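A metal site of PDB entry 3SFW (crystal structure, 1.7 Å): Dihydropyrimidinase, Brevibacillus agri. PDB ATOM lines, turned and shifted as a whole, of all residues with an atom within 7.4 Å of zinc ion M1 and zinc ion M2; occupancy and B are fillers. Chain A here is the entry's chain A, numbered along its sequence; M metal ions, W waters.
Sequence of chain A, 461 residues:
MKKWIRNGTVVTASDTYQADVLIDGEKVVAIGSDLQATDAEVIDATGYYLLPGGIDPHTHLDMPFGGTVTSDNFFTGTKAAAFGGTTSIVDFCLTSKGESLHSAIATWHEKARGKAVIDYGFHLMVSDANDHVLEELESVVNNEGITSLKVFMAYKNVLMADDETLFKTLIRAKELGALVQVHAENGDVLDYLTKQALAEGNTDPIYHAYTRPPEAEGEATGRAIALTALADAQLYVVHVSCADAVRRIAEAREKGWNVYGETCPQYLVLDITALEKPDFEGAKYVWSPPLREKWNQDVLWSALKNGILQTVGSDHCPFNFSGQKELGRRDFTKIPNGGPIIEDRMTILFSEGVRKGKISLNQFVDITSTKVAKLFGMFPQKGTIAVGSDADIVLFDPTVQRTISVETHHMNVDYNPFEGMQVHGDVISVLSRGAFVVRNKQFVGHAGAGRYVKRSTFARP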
ATOM      1  N   HIS A  58      21.877  22.394   5.822  1.00  0.00           N
ATOM      2  CA  HIS A  58      22.093  21.933   7.197  1.00  0.00           C
ATOM      3  C   HIS A  58      20.782  21.840   7.987  1.00  0.00           C
ATOM      4  O   HIS A  58      20.437  22.760   8.733  1.00  0.00           O
ATOM      5  CB  HIS A  58      23.141  22.797   7.902  1.00  0.00           C
ATOM      6  CG  HIS A  58      23.685  22.190   9.158  1.00  0.00           C
ATOM      7  ND1 HIS A  58      24.968  22.442   9.615  1.00  0.00           N
ATOM      8  CD2 HIS A  58      23.152  21.274  10.015  1.00  0.00           C
ATOM      9  CE1 HIS A  58      25.193  21.731  10.701  1.00  0.00           C
ATOM     10  NE2 HIS A  58      24.105  21.016  10.968  1.00  0.00           N
ATOM     11  N   THR A  59      20.033  20.751   7.774  1.00  0.00           N
ATOM     12  CA  THR A  59      18.735  20.610   8.489  1.00  0.00           C
ATOM     13  C   THR A  59      18.642  19.245   9.173  1.00  0.00           C
ATOM     14  O   THR A  59      19.330  18.301   8.791  1.00  0.00           O
ATOM     15  CB  THR A  59      17.520  20.808   7.557  1.00  0.00           C
ATOM     16  OG1 THR A  59      17.454  19.767   6.577  1.00  0.00           O
ATOM     17  CG2 THR A  59      17.678  22.173   6.778  1.00  0.00           C
ATOM     18  N   HIS A  60      17.815  19.174  10.215  1.00  0.00           N
ATOM     19  CA  HIS A  60      17.595  17.958  10.985  1.00  0.00           C
ATOM     20  C   HIS A  60      16.086  17.801  11.240  1.00  0.00           C
ATOM     21  O   HIS A  60      15.597  17.987  12.374  1.00  0.00           O
ATOM     22  CB  HIS A  60      18.336  18.045  12.340  1.00  0.00           C
ATOM     23  CG  HIS A  60      19.813  18.195  12.202  1.00  0.00           C
ATOM     24  ND1 HIS A  60      20.629  17.127  11.879  1.00  0.00           N
ATOM     25  CD2 HIS A  60      20.616  19.272  12.288  1.00  0.00           C
ATOM     26  CE1 HIS A  60      21.899  17.535  11.846  1.00  0.00           C
ATOM     27  NE2 HIS A  60      21.903  18.849  12.067  1.00  0.00           N
ATOM     28  N   MET A  63      14.183  14.416  13.452  1.00  0.00           N
ATOM     29  CA  MET A  63      15.417  13.754  13.853  1.00  0.00           C
ATOM     30  C   MET A  63      15.278  13.219  15.284  1.00  0.00           C
ATOM     31  O   MET A  63      14.977  13.971  16.200  1.00  0.00           O
ATOM     32  CB  MET A  63      16.553  14.789  13.851  1.00  0.00           C
ATOM     33  CG  MET A  63      17.923  14.189  14.305  1.00  0.00           C
ATOM     34  SD  MET A  63      18.945  15.526  14.976  1.00  0.00           S
ATOM     35  CE  MET A  63      20.507  14.767  15.205  1.00  0.00           C
ATOM     36  N   PHE A  65      16.854  12.609  18.681  1.00  0.00           N
ATOM     37  CA  PHE A  65      18.054  13.226  19.339  1.00  0.00           C
ATOM     38  C   PHE A  65      17.647  13.788  20.691  1.00  0.00           C
ATOM     39  O   PHE A  65      16.491  14.163  20.874  1.00  0.00           O
ATOM     40  CB  PHE A  65      18.597  14.374  18.448  1.00  0.00           C
ATOM     41  CG  PHE A  65      19.972  14.913  18.848  1.00  0.00           C
ATOM     42  CD1 PHE A  65      21.091  14.074  18.909  1.00  0.00           C
ATOM     43  CD2 PHE A  65      20.169  16.288  18.848  1.00  0.00           C
ATOM     44  CE1 PHE A  65      22.366  14.605  19.109  1.00  0.00           C
ATOM     45  CE2 PHE A  65      21.443  16.847  19.052  1.00  0.00           C
ATOM     46  CZ  PHE A  65      22.546  15.981  19.212  1.00  0.00           C
ATOM     47  N   PHE A  92      20.434  15.749   7.232  1.00  0.00           N
ATOM     48  CA  PHE A  92      21.313  14.663   7.688  1.00  0.00           C
ATOM     49  C   PHE A  92      20.606  13.342   8.001  1.00  0.00           C
ATOM     50  O   PHE A  92      19.977  13.181   9.076  1.00  0.00           O
ATOM     51  CB  PHE A  92      22.125  15.159   8.905  1.00  0.00           C
ATOM     52  CG  PHE A  92      23.156  16.190   8.538  1.00  0.00           C
ATOM     53  CD1 PHE A  92      22.882  17.556   8.661  1.00  0.00           C
ATOM     54  CD2 PHE A  92      24.389  15.806   8.090  1.00  0.00           C
ATOM     55  CE1 PHE A  92      23.805  18.502   8.325  1.00  0.00           C
ATOM     56  CE2 PHE A  92      25.334  16.757   7.717  1.00  0.00           C
ATOM     57  CZ  PHE A  92      25.031  18.125   7.812  1.00  0.00           C
ATOM     58  N   KCX A 150      28.867  12.816   6.650  1.00  0.00           N
ATOM     59  CA  KCX A 150      29.011  13.612   7.861  1.00  0.00           C
ATOM     60  CB  KCX A 150      27.573  14.000   8.347  1.00  0.00           C
ATOM     61  CG  KCX A 150      27.514  14.782   9.736  1.00  0.00           C
ATOM     62  CD  KCX A 150      28.297  16.173   9.638  1.00  0.00           C
ATOM     63  CE  KCX A 150      28.026  17.039  10.920  1.00  0.00           C
ATOM     64  NZ  KCX A 150      26.588  17.417  11.005  1.00  0.00           N
ATOM     65  C   KCX A 150      29.701  12.774   8.947  1.00  0.00           C
ATOM     66  O   KCX A 150      29.225  11.666   9.271  1.00  0.00           O
ATOM     67  CX  KCX A 150      26.090  18.137  12.020  1.00  0.00           C
ATOM     68  OQ1 KCX A 150      26.873  18.629  12.837  1.00  0.00           O
ATOM     69  OQ2 KCX A 150      24.852  18.331  12.085  1.00  0.00           O
ATOM     70  N   PHE A 152      30.758  13.071  12.966  1.00  0.00           N
ATOM     71  CA  PHE A 152      30.622  13.849  14.188  1.00  0.00           C
ATOM     72  C   PHE A 152      31.845  13.614  15.081  1.00  0.00           C
ATOM     73  O   PHE A 152      32.215  12.495  15.311  1.00  0.00           O
ATOM     74  CB  PHE A 152      29.328  13.399  14.931  1.00  0.00           C
ATOM     75  CG  PHE A 152      28.066  13.817  14.237  1.00  0.00           C
ATOM     76  CD1 PHE A 152      27.391  12.927  13.377  1.00  0.00           C
ATOM     77  CD2 PHE A 152      27.516  15.069  14.460  1.00  0.00           C
ATOM     78  CE1 PHE A 152      26.245  13.294  12.718  1.00  0.00           C
ATOM     79  CE2 PHE A 152      26.320  15.429  13.852  1.00  0.00           C
ATOM     80  CZ  PHE A 152      25.695  14.546  12.941  1.00  0.00           C
ATOM     81  N   TYR A 155      29.702  14.577  20.727  1.00  0.00           N
ATOM     82  CA  TYR A 155      28.559  13.715  21.137  1.00  0.00           C
ATOM     83  C   TYR A 155      29.005  12.291  21.436  1.00  0.00           C
ATOM     84  O   TYR A 155      28.501  11.321  20.882  1.00  0.00           O
ATOM     85  CB  TYR A 155      27.446  13.740  20.071  1.00  0.00           C
ATOM     86  CG  TYR A 155      26.961  15.127  19.709  1.00  0.00           C
ATOM     87  CD1 TYR A 155      26.323  15.959  20.633  1.00  0.00           C
ATOM     88  CD2 TYR A 155      27.104  15.590  18.410  1.00  0.00           C
ATOM     89  CE1 TYR A 155      25.868  17.250  20.246  1.00  0.00           C
ATOM     90  CE2 TYR A 155      26.650  16.853  18.021  1.00  0.00           C
ATOM     91  CZ  TYR A 155      26.052  17.667  18.931  1.00  0.00           C
ATOM     92  OH  TYR A 155      25.574  18.893  18.491  1.00  0.00           O
ATOM     93  N   LEU A 159      26.840  10.011  18.774  1.00  0.00           N
ATOM     94  CA  LEU A 159      27.129  10.184  17.316  1.00  0.00           C
ATOM     95  C   LEU A 159      28.617  10.139  17.021  1.00  0.00           C
ATOM     96  O   LEU A 159      29.022   9.973  15.876  1.00  0.00           O
ATOM     97  CB  LEU A 159      26.545  11.524  16.779  1.00  0.00           C
ATOM     98  CG  LEU A 159      25.062  11.832  17.019  1.00  0.00           C
ATOM     99  CD1 LEU A 159      24.704  13.217  16.412  1.00  0.00           C
ATOM    100  CD2 LEU A 159      24.178  10.708  16.397  1.00  0.00           C
ATOM    101  N   VAL A 182      32.391  17.766   8.674  1.00  0.00           N
ATOM    102  CA  VAL A 182      32.583  17.457  10.087  1.00  0.00           C
ATOM    103  C   VAL A 182      31.809  18.393  11.001  1.00  0.00           C
ATOM    104  O   VAL A 182      31.871  19.584  10.822  1.00  0.00           O
ATOM    105  CB  VAL A 182      34.086  17.491  10.458  1.00  0.00           C
ATOM    106  CG1 VAL A 182      34.280  17.629  11.890  1.00  0.00           C
ATOM    107  CG2 VAL A 182      34.798  16.255   9.897  1.00  0.00           C
ATOM    108  N   HIS A 183      31.294  17.827  12.098  1.00  0.00           N
ATOM    109  CA  HIS A 183      30.960  18.585  13.321  1.00  0.00           C
ATOM    110  C   HIS A 183      32.250  18.578  14.164  1.00  0.00           C
ATOM    111  O   HIS A 183      32.606  17.533  14.730  1.00  0.00           O
ATOM    112  CB  HIS A 183      29.805  17.898  14.116  1.00  0.00           C
ATOM    113  CG  HIS A 183      29.523  18.561  15.436  1.00  0.00           C
ATOM    114  ND1 HIS A 183      28.311  19.162  15.738  1.00  0.00           N
ATOM    115  CD2 HIS A 183      30.316  18.752  16.518  1.00  0.00           C
ATOM    116  CE1 HIS A 183      28.368  19.661  16.969  1.00  0.00           C
ATOM    117  NE2 HIS A 183      29.582  19.444  17.457  1.00  0.00           N
ATOM    118  N   ALA A 184      32.929  19.724  14.238  1.00  0.00           N
ATOM    119  CA  ALA A 184      34.305  19.734  14.780  1.00  0.00           C
ATOM    120  C   ALA A 184      34.307  20.338  16.191  1.00  0.00           C
ATOM    121  O   ALA A 184      34.621  21.531  16.370  1.00  0.00           O
ATOM    122  CB  ALA A 184      35.283  20.531  13.845  1.00  0.00           C
ATOM    123  N   GLU A 185      34.084  19.508  17.196  1.00  0.00           N
ATOM    124  CA  GLU A 185      34.479  19.855  18.599  1.00  0.00           C
ATOM    125  C   GLU A 185      35.135  18.602  19.140  1.00  0.00           C
ATOM    126  O   GLU A 185      34.676  17.477  18.828  1.00  0.00           O
ATOM    127  CB  GLU A 185      33.266  20.145  19.493  1.00  0.00           C
ATOM    128  CG  GLU A 185      32.385  21.349  19.062  1.00  0.00           C
ATOM    129  CD  GLU A 185      31.159  21.450  19.925  1.00  0.00           C
ATOM    130  OE1 GLU A 185      30.222  20.599  19.752  1.00  0.00           O
ATOM    131  OE2 GLU A 185      31.185  22.310  20.859  1.00  0.00           O
ATOM    132  N   VAL A 238      31.099  22.157   9.204  1.00  0.00           N
ATOM    133  CA  VAL A 238      29.751  22.725   9.385  1.00  0.00           C
ATOM    134  C   VAL A 238      29.797  23.643  10.619  1.00  0.00           C
ATOM    135  O   VAL A 238      30.726  23.565  11.425  1.00  0.00           O
ATOM    136  CB  VAL A 238      28.630  21.642   9.625  1.00  0.00           C
ATOM    137  CG1 VAL A 238      28.624  20.593   8.482  1.00  0.00           C
ATOM    138  CG2 VAL A 238      28.855  20.915  10.969  1.00  0.00           C
ATOM    139  N   HIS A 239      28.822  24.557  10.691  1.00  0.00           N
ATOM    140  CA  HIS A 239      28.688  25.498  11.809  1.00  0.00           C
ATOM    141  C   HIS A 239      30.021  25.924  12.430  1.00  0.00           C
ATOM    142  O   HIS A 239      30.244  25.707  13.618  1.00  0.00           O
ATOM    143  CB  HIS A 239      27.671  25.008  12.911  1.00  0.00           C
ATOM    144  CG  HIS A 239      27.878  23.595  13.413  1.00  0.00           C
ATOM    145  ND1 HIS A 239      29.101  23.108  13.840  1.00  0.00           N
ATOM    146  CD2 HIS A 239      26.962  22.622  13.682  1.00  0.00           C
ATOM    147  CE1 HIS A 239      28.942  21.861  14.286  1.00  0.00           C
ATOM    148  NE2 HIS A 239      27.659  21.557  14.212  1.00  0.00           N
ATOM    149  N   GLU A 262      31.189  26.545   6.669  1.00  0.00           N
ATOM    150  CA  GLU A 262      29.823  27.024   6.760  1.00  0.00           C
ATOM    151  C   GLU A 262      29.698  27.792   8.071  1.00  0.00           C
ATOM    152  O   GLU A 262      30.296  27.402   9.074  1.00  0.00           O
ATOM    153  CB  GLU A 262      28.940  25.782   6.901  1.00  0.00           C
ATOM    154  CG  GLU A 262      27.448  26.033   7.074  1.00  0.00           C
ATOM    155  CD  GLU A 262      26.767  24.691   7.400  1.00  0.00           C
ATOM    156  OE1 GLU A 262      26.690  24.333   8.611  1.00  0.00           O
ATOM    157  OE2 GLU A 262      26.405  23.966   6.434  1.00  0.00           O
ATOM    158  N   TYR A 267      25.211  32.120  15.051  1.00  0.00           N
ATOM    159  CA  TYR A 267      26.579  32.487  15.459  1.00  0.00           C
ATOM    160  C   TYR A 267      26.946  33.882  14.970  1.00  0.00           C
ATOM    161  O   TYR A 267      27.904  34.442  15.441  1.00  0.00           O
ATOM    162  CB  TYR A 267      27.604  31.436  14.995  1.00  0.00           C
ATOM    163  CG  TYR A 267      27.232  30.048  15.489  1.00  0.00           C
ATOM    164  CD1 TYR A 267      26.845  29.043  14.597  1.00  0.00           C
ATOM    165  CD2 TYR A 267      27.241  29.771  16.877  1.00  0.00           C
ATOM    166  CE1 TYR A 267      26.451  27.781  15.038  1.00  0.00           C
ATOM    167  CE2 TYR A 267      26.890  28.503  17.330  1.00  0.00           C
ATOM    168  CZ  TYR A 267      26.501  27.506  16.427  1.00  0.00           C
ATOM    169  OH  TYR A 267      26.162  26.248  16.913  1.00  0.00           O
ATOM    170  N   SER A 288      24.882  23.212  19.733  1.00  0.00           N
ATOM    171  CA  SER A 288      26.343  23.003  19.796  1.00  0.00           C
ATOM    172  C   SER A 288      26.896  23.164  18.397  1.00  0.00           C
ATOM    173  O   SER A 288      26.214  22.817  17.461  1.00  0.00           O
ATOM    174  CB  SER A 288      26.650  21.576  20.266  1.00  0.00           C
ATOM    175  OG  SER A 288      26.143  21.383  21.586  1.00  0.00           O
ATOM    176  N   PRO A 289      28.083  23.754  18.249  1.00  0.00           N
ATOM    177  CA  PRO A 289      28.872  24.452  19.263  1.00  0.00           C
ATOM    178  C   PRO A 289      28.082  25.533  19.904  1.00  0.00           C
ATOM    179  O   PRO A 289      27.102  26.014  19.357  1.00  0.00           O
ATOM    180  CB  PRO A 289      30.039  25.059  18.477  1.00  0.00           C
ATOM    181  CG  PRO A 289      29.542  25.124  17.056  1.00  0.00           C
ATOM    182  CD  PRO A 289      28.686  23.911  16.899  1.00  0.00           C
ATOM    183  N   SER A 314      21.384  26.549   8.396  1.00  0.00           N
ATOM    184  CA  SER A 314      20.653  26.906   9.647  1.00  0.00           C
ATOM    185  C   SER A 314      21.060  25.996  10.832  1.00  0.00           C
ATOM    186  O   SER A 314      21.027  26.466  11.981  1.00  0.00           O
ATOM    187  CB  SER A 314      19.127  26.800   9.452  1.00  0.00           C
ATOM    188  OG  SER A 314      18.782  25.474   9.063  1.00  0.00           O
ATOM    189  N   ASP A 315      21.393  24.713  10.570  1.00  0.00           N
ATOM    190  CA  ASP A 315      21.424  23.682  11.656  1.00  0.00           C
ATOM    191  C   ASP A 315      20.040  23.676  12.357  1.00  0.00           C
ATOM    192  O   ASP A 315      19.920  23.583  13.605  1.00  0.00           O
ATOM    193  CB  ASP A 315      22.595  23.857  12.680  1.00  0.00           C
ATOM    194  CG  ASP A 315      22.833  22.637  13.553  1.00  0.00           C
ATOM    195  OD1 ASP A 315      22.405  21.509  13.151  1.00  0.00           O
ATOM    196  OD2 ASP A 315      23.427  22.811  14.666  1.00  0.00           O
ATOM    197  N   HIS A 316      19.000  23.730  11.548  1.00  0.00           N
ATOM    198  CA  HIS A 316      17.622  23.711  12.112  1.00  0.00           C
ATOM    199  C   HIS A 316      17.430  22.380  12.843  1.00  0.00           C
ATOM    200  O   HIS A 316      17.480  21.305  12.242  1.00  0.00           O
ATOM    201  CB  HIS A 316      16.594  23.789  10.978  1.00  0.00           C
ATOM    202  CG  HIS A 316      15.184  23.906  11.471  1.00  0.00           C
ATOM    203  ND1 HIS A 316      14.764  24.971  12.235  1.00  0.00           N
ATOM    204  CD2 HIS A 316      14.115  23.108  11.295  1.00  0.00           C
ATOM    205  CE1 HIS A 316      13.485  24.823  12.528  1.00  0.00           C
ATOM    206  NE2 HIS A 316      13.065  23.685  11.974  1.00  0.00           N
ATOM    207  N   CYS A 317      17.166  22.446  14.151  1.00  0.00           N
ATOM    208  CA  CYS A 317      17.126  21.225  14.950  1.00  0.00           C
ATOM    209  C   CYS A 317      16.184  21.572  16.160  1.00  0.00           C
ATOM    210  O   CYS A 317      16.634  21.667  17.298  1.00  0.00           O
ATOM    211  CB  CYS A 317      18.568  20.885  15.394  1.00  0.00           C
ATOM    212  SG  CYS A 317      18.738  19.201  16.140  1.00  0.00           S
HETATM  213 ZN    ZN M   1      23.655  19.843  12.707  1.00  0.00          ZN
HETATM  214 ZN    ZN M   2      26.524  19.724  14.576  1.00  0.00          ZN
HETATM  215  O   HOH W   1      25.248  18.209  15.297  1.00  0.00           O
HETATM  216  O   HOH W   2      25.468  20.495  16.396  1.00  0.00           O
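The backbone carbonyl oxygen (O) of His 58 lies within hydrogen-bond range of the backbone NH (N) of His 316 (3.3 Å). The side-chain carboxylate (OE1) of Glu 262 sits at hydrogen-bond distance from a ring nitrogen (ND1) of His 58. The backbone carbonyl oxygen (O) of His 58 sits at hydrogen-bond distance from the side-chain hydroxyl (OG) of Ser 314 (3.2 Å). The side-chain carboxylate of Glu 262 sits at hydrogen-bond distance from the backbone NH of His 239 (3.0 Å). OE1 of Glu 185 lies within hydrogen-bond range of NE2 of His 183 (2.6 Å). The backbone NH (N) of His 60 lies within hydrogen-bond range of the backbone carbonyl oxygen (O) of His 316.
Of the 24 residues printed, 4 come within 4 Å of zinc ion M1.
Three residues have an atom within 4 Å of zinc ion M2: KCX 150, His 183 and His 239. The nearest printed residue that does not touch zinc ion M2 is Tyr 155 (4.1 Å).
Zinc ion M1 is bound by OQ2 of KCX 150 (2.0 Å), a ring nitrogen (NE2) of His 60 (2.1 Å), the side-chain carboxylate (OD1) of Asp 315 (2.1 Å) and a ring nitrogen (NE2) of His 58 (2.1 Å).
Zinc ion M2 is bound by OQ1 of KCX 150 (2.1 Å), water W1 (2.1 Å), NE2 of His 239 (2.2 Å), ND1 of His 183 (2.2 Å) and water W2 (2.2 Å).
Water W2 lies within hydrogen-bond range of OH of Tyr 155 (2.6 Å) and O of Ser 288 (2.7 Å).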
